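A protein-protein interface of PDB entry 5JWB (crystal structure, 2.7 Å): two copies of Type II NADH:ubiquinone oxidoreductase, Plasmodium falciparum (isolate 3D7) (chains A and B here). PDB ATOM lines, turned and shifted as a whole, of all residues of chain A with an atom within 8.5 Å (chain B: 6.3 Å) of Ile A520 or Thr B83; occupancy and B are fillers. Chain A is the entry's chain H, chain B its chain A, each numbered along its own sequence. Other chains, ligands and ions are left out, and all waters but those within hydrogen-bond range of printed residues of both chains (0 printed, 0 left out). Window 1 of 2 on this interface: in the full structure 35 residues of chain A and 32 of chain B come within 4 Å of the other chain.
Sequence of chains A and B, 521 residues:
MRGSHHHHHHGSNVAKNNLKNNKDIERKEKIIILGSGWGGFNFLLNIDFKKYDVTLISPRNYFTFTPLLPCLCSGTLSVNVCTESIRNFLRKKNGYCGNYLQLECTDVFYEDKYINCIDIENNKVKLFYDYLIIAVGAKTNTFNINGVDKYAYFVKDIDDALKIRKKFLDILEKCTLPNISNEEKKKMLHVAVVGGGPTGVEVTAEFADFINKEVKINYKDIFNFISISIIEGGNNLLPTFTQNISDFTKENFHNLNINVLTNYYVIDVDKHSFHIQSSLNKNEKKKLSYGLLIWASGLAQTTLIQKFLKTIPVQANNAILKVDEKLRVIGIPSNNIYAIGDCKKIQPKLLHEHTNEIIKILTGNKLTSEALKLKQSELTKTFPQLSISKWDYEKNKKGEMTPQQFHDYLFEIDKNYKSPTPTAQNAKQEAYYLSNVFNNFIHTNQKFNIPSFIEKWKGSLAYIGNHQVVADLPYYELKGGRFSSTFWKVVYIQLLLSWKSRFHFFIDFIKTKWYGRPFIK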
ATOM      1  N   GLY A  75     -24.360 -36.713  13.077  1.00  0.00           N
ATOM      2  CA  GLY A  75     -23.533 -35.529  12.915  1.00  0.00           C
ATOM      3  C   GLY A  75     -22.124 -35.622  13.478  1.00  0.00           C
ATOM      4  O   GLY A  75     -21.383 -34.637  13.482  1.00  0.00           O
ATOM      5  N   LEU A 162     -28.490 -38.325   5.751  1.00  0.00           N
ATOM      6  CA  LEU A 162     -28.818 -36.914   5.907  1.00  0.00           C
ATOM      7  C   LEU A 162     -30.324 -36.671   6.039  1.00  0.00           C
ATOM      8  O   LEU A 162     -30.759 -35.819   6.833  1.00  0.00           O
ATOM      9  CB  LEU A 162     -28.269 -36.119   4.732  1.00  0.00           C
ATOM     10  CG  LEU A 162     -26.751 -36.203   4.616  1.00  0.00           C
ATOM     11  CD1 LEU A 162     -26.257 -35.369   3.441  1.00  0.00           C
ATOM     12  CD2 LEU A 162     -26.114 -35.766   5.927  1.00  0.00           C
ATOM     13  N   ARG A 165     -31.122 -37.638   9.546  1.00  0.00           N
ATOM     14  CA  ARG A 165     -30.666 -36.593  10.468  1.00  0.00           C
ATOM     15  C   ARG A 165     -31.605 -35.393  10.462  1.00  0.00           C
ATOM     16  O   ARG A 165     -31.978 -34.882  11.527  1.00  0.00           O
ATOM     17  CB  ARG A 165     -29.258 -36.134  10.122  1.00  0.00           C
ATOM     18  CG  ARG A 165     -28.630 -35.210  11.157  1.00  0.00           C
ATOM     19  CD  ARG A 165     -27.238 -34.735  10.702  1.00  0.00           C
ATOM     20  NE  ARG A 165     -26.828 -33.504  11.377  1.00  0.00           N
ATOM     21  CZ  ARG A 165     -27.232 -32.283  11.024  1.00  0.00           C
ATOM     22  NH1 ARG A 165     -28.059 -32.130   9.993  1.00  0.00           N
ATOM     23  NH2 ARG A 165     -26.817 -31.213  11.699  1.00  0.00           N
ATOM     24  N   LYS A 166     -31.998 -34.955   9.266  1.00  0.00           N
ATOM     25  CA  LYS A 166     -32.898 -33.806   9.157  1.00  0.00           C
ATOM     26  C   LYS A 166     -34.270 -34.052   9.821  1.00  0.00           C
ATOM     27  O   LYS A 166     -34.753 -33.236  10.603  1.00  0.00           O
ATOM     28  CB  LYS A 166     -33.104 -33.411   7.692  1.00  0.00           C
ATOM     29  CG  LYS A 166     -34.128 -32.314   7.577  1.00  0.00           C
ATOM     30  CD  LYS A 166     -34.044 -31.492   6.311  1.00  0.00           C
ATOM     31  CE  LYS A 166     -35.028 -30.323   6.390  1.00  0.00           C
ATOM     32  NZ  LYS A 166     -36.437 -30.820   6.437  1.00  0.00           N
ATOM     33  N   LEU A 169     -34.168 -33.700  13.505  1.00  0.00           N
ATOM     34  CA  LEU A 169     -34.032 -32.326  13.966  1.00  0.00           C
ATOM     35  C   LEU A 169     -35.325 -31.563  13.681  1.00  0.00           C
ATOM     36  O   LEU A 169     -35.743 -30.713  14.463  1.00  0.00           O
ATOM     37  CB  LEU A 169     -32.821 -31.657  13.300  1.00  0.00           C
ATOM     38  CG  LEU A 169     -31.501 -32.408  13.530  1.00  0.00           C
ATOM     39  CD1 LEU A 169     -30.326 -31.805  12.746  1.00  0.00           C
ATOM     40  CD2 LEU A 169     -31.179 -32.514  15.025  1.00  0.00           C
ATOM     41  N   ASP A 170     -35.964 -31.890  12.564  1.00  0.00           N
ATOM     42  CA  ASP A 170     -37.276 -31.354  12.269  1.00  0.00           C
ATOM     43  C   ASP A 170     -38.248 -31.644  13.395  1.00  0.00           C
ATOM     44  O   ASP A 170     -39.016 -30.773  13.791  1.00  0.00           O
ATOM     45  CB  ASP A 170     -37.835 -31.942  10.979  1.00  0.00           C
ATOM     46  CG  ASP A 170     -37.354 -31.217   9.744  1.00  0.00           C
ATOM     47  OD1 ASP A 170     -37.535 -31.780   8.633  1.00  0.00           O
ATOM     48  OD2 ASP A 170     -36.803 -30.101   9.877  1.00  0.00           O
ATOM     49  N   PHE A 210     -26.277 -38.854  20.584  1.00  0.00           N
ATOM     50  CA  PHE A 210     -26.712 -37.517  20.216  1.00  0.00           C
ATOM     51  C   PHE A 210     -27.794 -37.032  21.175  1.00  0.00           C
ATOM     52  O   PHE A 210     -27.743 -35.896  21.685  1.00  0.00           O
ATOM     53  CB  PHE A 210     -27.224 -37.513  18.778  1.00  0.00           C
ATOM     54  CG  PHE A 210     -27.413 -36.145  18.198  1.00  0.00           C
ATOM     55  CD1 PHE A 210     -26.769 -35.052  18.735  1.00  0.00           C
ATOM     56  CD2 PHE A 210     -28.249 -35.960  17.118  1.00  0.00           C
ATOM     57  CE1 PHE A 210     -26.949 -33.801  18.195  1.00  0.00           C
ATOM     58  CE2 PHE A 210     -28.429 -34.725  16.573  1.00  0.00           C
ATOM     59  CZ  PHE A 210     -27.783 -33.640  17.107  1.00  0.00           C
ATOM     60  N   TYR A 219     -32.410 -29.132  24.401  1.00  0.00           N
ATOM     61  CA  TYR A 219     -33.841 -29.352  24.435  1.00  0.00           C
ATOM     62  C   TYR A 219     -34.293 -29.963  25.767  1.00  0.00           C
ATOM     63  O   TYR A 219     -35.020 -30.964  25.759  1.00  0.00           O
ATOM     64  CB  TYR A 219     -34.264 -30.269  23.294  1.00  0.00           C
ATOM     65  CG  TYR A 219     -33.932 -29.797  21.893  1.00  0.00           C
ATOM     66  CD1 TYR A 219     -34.890 -29.170  21.114  1.00  0.00           C
ATOM     67  CD2 TYR A 219     -32.675 -30.026  21.325  1.00  0.00           C
ATOM     68  CE1 TYR A 219     -34.615 -28.765  19.814  1.00  0.00           C
ATOM     69  CE2 TYR A 219     -32.384 -29.614  20.010  1.00  0.00           C
ATOM     70  CZ  TYR A 219     -33.366 -28.981  19.263  1.00  0.00           C
ATOM     71  OH  TYR A 219     -33.120 -28.559  17.965  1.00  0.00           O
ATOM     72  N   ARG A 517     -21.743 -31.867  18.233  1.00  0.00           N
ATOM     73  CA  ARG A 517     -22.481 -32.119  17.013  1.00  0.00           C
ATOM     74  C   ARG A 517     -23.294 -30.893  16.604  1.00  0.00           C
ATOM     75  O   ARG A 517     -23.725 -30.132  17.463  1.00  0.00           O
ATOM     76  CB  ARG A 517     -23.377 -33.340  17.213  1.00  0.00           C
ATOM     77  CG  ARG A 517     -22.569 -34.613  17.446  1.00  0.00           C
ATOM     78  CD  ARG A 517     -23.437 -35.785  17.872  1.00  0.00           C
ATOM     79  NE  ARG A 517     -22.608 -36.949  18.151  1.00  0.00           N
ATOM     80  CZ  ARG A 517     -22.280 -37.352  19.371  1.00  0.00           C
ATOM     81  NH1 ARG A 517     -22.735 -36.696  20.429  1.00  0.00           N
ATOM     82  NH2 ARG A 517     -21.509 -38.420  19.525  1.00  0.00           N
ATOM     83  N   PRO A 518     -23.468 -30.682  15.286  1.00  0.00           N
ATOM     84  CA  PRO A 518     -24.207 -29.528  14.754  1.00  0.00           C
ATOM     85  C   PRO A 518     -25.721 -29.746  14.648  1.00  0.00           C
ATOM     86  O   PRO A 518     -26.153 -30.885  14.543  1.00  0.00           O
ATOM     87  CB  PRO A 518     -23.585 -29.335  13.360  1.00  0.00           C
ATOM     88  CG  PRO A 518     -23.102 -30.683  12.961  1.00  0.00           C
ATOM     89  CD  PRO A 518     -22.711 -31.395  14.232  1.00  0.00           C
ATOM     90  N   PHE A 519     -26.503 -28.664  14.658  1.00  0.00           N
ATOM     91  CA  PHE A 519     -27.958 -28.741  14.457  1.00  0.00           C
ATOM     92  C   PHE A 519     -28.474 -28.181  13.117  1.00  0.00           C
ATOM     93  O   PHE A 519     -29.687 -28.151  12.892  1.00  0.00           O
ATOM     94  CB  PHE A 519     -28.681 -28.019  15.591  1.00  0.00           C
ATOM     95  CG  PHE A 519     -28.622 -28.741  16.888  1.00  0.00           C
ATOM     96  CD1 PHE A 519     -29.447 -29.824  17.126  1.00  0.00           C
ATOM     97  CD2 PHE A 519     -27.731 -28.352  17.868  1.00  0.00           C
ATOM     98  CE1 PHE A 519     -29.394 -30.499  18.325  1.00  0.00           C
ATOM     99  CE2 PHE A 519     -27.669 -29.031  19.072  1.00  0.00           C
ATOM    100  CZ  PHE A 519     -28.501 -30.109  19.296  1.00  0.00           C
ATOM    101  N   ILE A 520     -27.569 -27.740  12.245  1.00  0.00           N
ATOM    102  CA  ILE A 520     -27.925 -27.287  10.898  1.00  0.00           C
ATOM    103  C   ILE A 520     -28.791 -28.304  10.132  1.00  0.00           C
ATOM    104  O   ILE A 520     -28.444 -29.488  10.093  1.00  0.00           O
ATOM    105  CB  ILE A 520     -26.649 -27.006  10.068  1.00  0.00           C
ATOM    106  CG1 ILE A 520     -25.632 -26.284  10.929  1.00  0.00           C
ATOM    107  CG2 ILE A 520     -26.959 -26.124   8.854  1.00  0.00           C
ATOM    108  CD1 ILE A 520     -26.094 -24.892  11.297  1.00  0.00           C
ATOM    109  N   LYS A 521     -29.892 -27.853   9.516  1.00  0.00           N
ATOM    110  CA  LYS A 521     -30.749 -28.775   8.752  1.00  0.00           C
ATOM    111  C   LYS A 521     -31.407 -28.169   7.500  1.00  0.00           C
ATOM    112  O   LYS A 521     -31.808 -27.006   7.484  1.00  0.00           O
ATOM    113  CB  LYS A 521     -31.835 -29.361   9.666  1.00  0.00           C
ATOM    114  CG  LYS A 521     -32.839 -28.354  10.207  1.00  0.00           C
ATOM    115  CD  LYS A 521     -33.599 -28.927  11.384  1.00  0.00           C
ATOM    116  CE  LYS A 521     -34.796 -28.063  11.798  1.00  0.00           C
ATOM    117  NZ  LYS A 521     -35.892 -28.062  10.780  1.00  0.00           N
ATOM    118  N   ASN B  61     -33.276 -22.232  11.330  1.00  0.00           N
ATOM    119  CA  ASN B  61     -32.813 -22.500  12.692  1.00  0.00           C
ATOM    120  C   ASN B  61     -31.322 -22.263  12.864  1.00  0.00           C
ATOM    121  O   ASN B  61     -30.713 -22.668  13.853  1.00  0.00           O
ATOM    122  CB  ASN B  61     -33.185 -23.930  13.112  1.00  0.00           C
ATOM    123  CG  ASN B  61     -32.164 -24.970  12.673  1.00  0.00           C
ATOM    124  OD1 ASN B  61     -31.631 -24.917  11.567  1.00  0.00           O
ATOM    125  ND2 ASN B  61     -31.907 -25.945  13.546  1.00  0.00           N
ATOM    126  N   TYR B  62     -30.734 -21.575  11.903  1.00  0.00           N
ATOM    127  CA  TYR B  62     -29.335 -21.211  12.010  1.00  0.00           C
ATOM    128  C   TYR B  62     -29.113 -19.784  11.542  1.00  0.00           C
ATOM    129  O   TYR B  62     -29.948 -19.208  10.825  1.00  0.00           O
ATOM    130  CB  TYR B  62     -28.463 -22.160  11.192  1.00  0.00           C
ATOM    131  CG  TYR B  62     -28.932 -22.345   9.766  1.00  0.00           C
ATOM    132  CD1 TYR B  62     -28.453 -21.533   8.745  1.00  0.00           C
ATOM    133  CD2 TYR B  62     -29.863 -23.336   9.440  1.00  0.00           C
ATOM    134  CE1 TYR B  62     -28.880 -21.705   7.431  1.00  0.00           C
ATOM    135  CE2 TYR B  62     -30.294 -23.511   8.139  1.00  0.00           C
ATOM    136  CZ  TYR B  62     -29.798 -22.691   7.139  1.00  0.00           C
ATOM    137  OH  TYR B  62     -30.231 -22.864   5.844  1.00  0.00           O
ATOM    138  N   PHE B  63     -27.989 -19.222  11.969  1.00  0.00           N
ATOM    139  CA  PHE B  63     -27.499 -17.979  11.410  1.00  0.00           C
ATOM    140  C   PHE B  63     -26.605 -18.294  10.206  1.00  0.00           C
ATOM    141  O   PHE B  63     -25.774 -19.207  10.247  1.00  0.00           O
ATOM    142  CB  PHE B  63     -26.736 -17.170  12.454  1.00  0.00           C
ATOM    143  CG  PHE B  63     -25.819 -16.127  11.865  1.00  0.00           C
ATOM    144  CD1 PHE B  63     -26.320 -14.899  11.444  1.00  0.00           C
ATOM    145  CD2 PHE B  63     -24.452 -16.370  11.748  1.00  0.00           C
ATOM    146  CE1 PHE B  63     -25.479 -13.937  10.924  1.00  0.00           C
ATOM    147  CE2 PHE B  63     -23.604 -15.418  11.230  1.00  0.00           C
ATOM    148  CZ  PHE B  63     -24.118 -14.197  10.818  1.00  0.00           C
ATOM    149  N   THR B  64     -26.792 -17.542   9.131  1.00  0.00           N
ATOM    150  CA  THR B  64     -26.007 -17.747   7.940  1.00  0.00           C
ATOM    151  C   THR B  64     -24.991 -16.614   7.794  1.00  0.00           C
ATOM    152  O   THR B  64     -25.360 -15.457   7.667  1.00  0.00           O
ATOM    153  CB  THR B  64     -26.902 -17.849   6.678  1.00  0.00           C
ATOM    154  OG1 THR B  64     -26.059 -17.829   5.517  1.00  0.00           O
ATOM    155  N   PHE B  65     -23.711 -16.961   7.834  1.00  0.00           N
ATOM    156  CA  PHE B  65     -22.634 -15.996   7.700  1.00  0.00           C
ATOM    157  C   PHE B  65     -22.438 -15.645   6.218  1.00  0.00           C
ATOM    158  O   PHE B  65     -21.525 -16.164   5.560  1.00  0.00           O
ATOM    159  CB  PHE B  65     -21.344 -16.567   8.318  1.00  0.00           C
ATOM    160  CG  PHE B  65     -20.229 -15.557   8.472  1.00  0.00           C
ATOM    161  CD1 PHE B  65     -20.095 -14.818   9.644  1.00  0.00           C
ATOM    162  CD2 PHE B  65     -19.314 -15.345   7.447  1.00  0.00           C
ATOM    163  CE1 PHE B  65     -19.061 -13.896   9.803  1.00  0.00           C
ATOM    164  CE2 PHE B  65     -18.282 -14.414   7.593  1.00  0.00           C
ATOM    165  CZ  PHE B  65     -18.157 -13.691   8.774  1.00  0.00           C
ATOM    166  N   SER B  78     -16.820 -24.977   3.784  1.00  0.00           N
ATOM    167  CA  SER B  78     -17.913 -25.899   4.076  1.00  0.00           C
ATOM    168  C   SER B  78     -19.108 -25.201   4.700  1.00  0.00           C
ATOM    169  O   SER B  78     -19.067 -24.010   4.989  1.00  0.00           O
ATOM    170  CB  SER B  78     -17.430 -26.985   5.007  1.00  0.00           C
ATOM    171  OG  SER B  78     -17.208 -26.435   6.294  1.00  0.00           O
ATOM    172  N   VAL B  79     -20.170 -25.951   4.937  1.00  0.00           N
ATOM    173  CA  VAL B  79     -21.361 -25.377   5.535  1.00  0.00           C
ATOM    174  C   VAL B  79     -21.081 -24.964   6.977  1.00  0.00           C
ATOM    175  O   VAL B  79     -21.617 -23.968   7.476  1.00  0.00           O
ATOM    176  CB  VAL B  79     -22.533 -26.363   5.480  1.00  0.00           C
ATOM    177  CG1 VAL B  79     -23.723 -25.808   6.194  1.00  0.00           C
ATOM    178  CG2 VAL B  79     -22.898 -26.641   4.040  1.00  0.00           C
ATOM    179  N   ASN B  80     -20.209 -25.709   7.640  1.00  0.00           N
ATOM    180  CA  ASN B  80     -19.917 -25.444   9.040  1.00  0.00           C
ATOM    181  C   ASN B  80     -19.333 -24.063   9.290  1.00  0.00           C
ATOM    182  O   ASN B  80     -19.584 -23.460  10.327  1.00  0.00           O
ATOM    183  CB  ASN B  80     -18.973 -26.505   9.580  1.00  0.00           C
ATOM    184  CG  ASN B  80     -19.579 -27.891   9.521  1.00  0.00           C
ATOM    185  OD1 ASN B  80     -20.541 -28.178  10.234  1.00  0.00           O
ATOM    186  ND2 ASN B  80     -19.022 -28.760   8.675  1.00  0.00           N
ATOM    187  N   VAL B  81     -18.564 -23.549   8.342  1.00  0.00           N
ATOM    188  CA  VAL B  81     -17.947 -22.254   8.540  1.00  0.00           C
ATOM    189  C   VAL B  81     -18.928 -21.127   8.205  1.00  0.00           C
ATOM    190  O   VAL B  81     -18.760 -20.005   8.662  1.00  0.00           O
ATOM    191  CB  VAL B  81     -16.659 -22.123   7.707  1.00  0.00           C
ATOM    192  CG1 VAL B  81     -16.984 -22.110   6.230  1.00  0.00           C
ATOM    193  CG2 VAL B  81     -15.886 -20.878   8.105  1.00  0.00           C
ATOM    194  N   CYS B  82     -19.975 -21.432   7.447  1.00  0.00           N
ATOM    195  CA  CYS B  82     -20.972 -20.420   7.066  1.00  0.00           C
ATOM    196  C   CYS B  82     -22.170 -20.406   7.991  1.00  0.00           C
ATOM    197  O   CYS B  82     -23.177 -19.771   7.693  1.00  0.00           O
ATOM    198  CB  CYS B  82     -21.479 -20.659   5.638  1.00  0.00           C
ATOM    199  SG  CYS B  82     -20.206 -20.714   4.400  1.00  0.00           S
ATOM    200  N   THR B  83     -22.073 -21.116   9.105  1.00  0.00           N
ATOM    201  CA  THR B  83     -23.244 -21.389   9.906  1.00  0.00           C
ATOM    202  C   THR B  83     -22.993 -21.199  11.378  1.00  0.00           C
ATOM    203  O   THR B  83     -21.886 -21.454  11.861  1.00  0.00           O
ATOM    204  CB  THR B  83     -23.731 -22.832   9.674  1.00  0.00           C
ATOM    205  OG1 THR B  83     -24.626 -22.839   8.553  1.00  0.00           O
ATOM    206  N   GLU B  84     -24.030 -20.757  12.082  1.00  0.00           N
ATOM    207  CA  GLU B  84     -24.122 -20.903  13.539  1.00  0.00           C
ATOM    208  C   GLU B  84     -25.512 -21.418  13.920  1.00  0.00           C
ATOM    209  O   GLU B  84     -26.513 -20.863  13.480  1.00  0.00           O
ATOM    210  CB  GLU B  84     -23.841 -19.578  14.245  1.00  0.00           C
ATOM    211  CG  GLU B  84     -22.500 -18.984  13.927  1.00  0.00           C
ATOM    212  CD  GLU B  84     -21.363 -19.718  14.610  1.00  0.00           C
ATOM    213  OE1 GLU B  84     -20.215 -19.289  14.389  1.00  0.00           O
ATOM    214  OE2 GLU B  84     -21.600 -20.707  15.363  1.00  0.00           O
ATOM    215  N   SER B  85     -25.586 -22.489  14.704  1.00  0.00           N
ATOM    216  CA  SER B  85     -26.883 -23.000  15.163  1.00  0.00           C
ATOM    217  C   SER B  85     -27.410 -22.145  16.303  1.00  0.00           C
ATOM    218  O   SER B  85     -26.725 -21.997  17.322  1.00  0.00           O
ATOM    219  CB  SER B  85     -26.780 -24.449  15.633  1.00  0.00           C
ATOM    220  OG  SER B  85     -26.405 -25.320  14.577  1.00  0.00           O
ATOM    221  N   ILE B 158     -27.734 -20.619   2.395  1.00  0.00           N
ATOM    222  CA  ILE B 158     -26.982 -21.867   2.316  1.00  0.00           C
ATOM    223  C   ILE B 158     -27.525 -22.802   1.239  1.00  0.00           C
ATOM    224  O   ILE B 158     -26.768 -23.346   0.418  1.00  0.00           O
ATOM    225  CB  ILE B 158     -27.006 -22.621   3.664  1.00  0.00           C
ATOM    226  CG1 ILE B 158     -26.463 -21.733   4.780  1.00  0.00           C
ATOM    227  CG2 ILE B 158     -26.242 -23.929   3.566  1.00  0.00           C
ATOM    228  CD1 ILE B 158     -25.066 -21.329   4.578  1.00  0.00           C
ATOM    229  N   SER B 498     -17.860 -17.335  16.295  1.00  0.00           N
ATOM    230  CA  SER B 498     -17.557 -18.405  17.229  1.00  0.00           C
ATOM    231  C   SER B 498     -16.168 -18.966  16.970  1.00  0.00           C
ATOM    232  O   SER B 498     -15.626 -18.799  15.880  1.00  0.00           O
ATOM    233  CB  SER B 498     -18.607 -19.511  17.137  1.00  0.00           C
ATOM    234  OG  SER B 498     -18.509 -20.241  15.929  1.00  0.00           O
ATOM    235  N   LYS B 500     -15.699 -22.150  17.003  1.00  0.00           N
ATOM    236  CA  LYS B 500     -16.009 -23.300  16.169  1.00  0.00           C
ATOM    237  C   LYS B 500     -15.786 -22.921  14.718  1.00  0.00           C
ATOM    238  O   LYS B 500     -15.102 -23.615  13.975  1.00  0.00           O
ATOM    239  CB  LYS B 500     -17.456 -23.786  16.361  1.00  0.00           C
ATOM    240  CG  LYS B 500     -17.904 -24.733  15.238  1.00  0.00           C
ATOM    241  CD  LYS B 500     -19.393 -24.703  15.029  1.00  0.00           C
ATOM    242  CE  LYS B 500     -19.875 -23.362  14.478  1.00  0.00           C
ATOM    243  NZ  LYS B 500     -20.008 -23.286  13.013  1.00  0.00           N
ATOM    244  N   SER B 501     -16.371 -21.807  14.325  1.00  0.00           N
ATOM    245  CA  SER B 501     -16.285 -21.392  12.950  1.00  0.00           C
ATOM    246  C   SER B 501     -14.857 -21.019  12.556  1.00  0.00           C
ATOM    247  O   SER B 501     -14.470 -21.165  11.386  1.00  0.00           O
ATOM    248  CB  SER B 501     -17.245 -20.240  12.707  1.00  0.00           C
ATOM    249  OG  SER B 501     -18.564 -20.736  12.747  1.00  0.00           O
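ND2 of Asn B61 is in hydrogen-bond range of O of Phe A519 (3.2 Å). OG of Ser B85 sits at hydrogen-bond distance from N of Phe A519 (3.3 Å).
No position is printed for both chains.
Ile A520 touches Tyr B62. CB of Thr B83 touches CD1 of Ile A520 (3.5 Å). Ile A520 touches Ser B85. Lys A521 touches Asn B61. CE2 of Tyr B62 touches O of Lys A521, at 3.9 Å.
Gly A75 touches none of the printed residues of chain B. Of the printed residues of chain B, Phe A519 touches Asn B61 (3.2 Å) and Ser B85 (3.3 Å). Of chain B, only Tyr B62, Thr B83 and Ser B85 come within 4 Å of Ile A520. Of the printed residues of chain B, Lys A521 touches Asn B61 and Tyr B62. Of the printed residues of chain A, Asn B61 touches Phe A519 and Lys A521. Printed residues of chain A within 4 Å of Tyr B62: Ile A520 and Lys A521. Of chain A, only Ile A520 comes within 4 Å of Thr B83. Of the printed residues of chain A, Ser B85 touches Phe A519 (3.3 Å) and Ile A520 (3.3 Å). The nearest residue of chain A that does not touch Thr B83 is Lys A521 (7.3 Å). The nearest printed residue of chain B that does not touch Phe A519 is Tyr B62 (5.9 Å).
Hydrophobic or aromatic side chains of chain B within 4 Å of the printed part of chain A: Tyr B62. Of the 13 printed residues of chain A, 3 touch a printed residue of chain B. Hydrophobic or aromatic side chains of chain A within 4 Å of the printed part of chain B: Phe A519 and Ile A520. Along chain A the printed residues that touch a printed residue of chain B span positions 519 to 521. Among the printed residues, 7 pairs touch across the chains. Among the printed residues, no Asp or Glu carboxylate lies within 4 Å of a Lys or Arg side-chain nitrogen of the other chain.
OG1 of Thr B83 lies close to O of Val B79 (3.4 Å). O of Thr B83 sits at hydrogen-bond distance from NZ of Lys B500, 2.9 Å away. NH1 of Arg A165 is in hydrogen-bond range of O of Ile A520 (2.7 Å). NZ of Lys A521 is in salt-bridge range of OD2 of Asp A170, 2.4 Å away.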
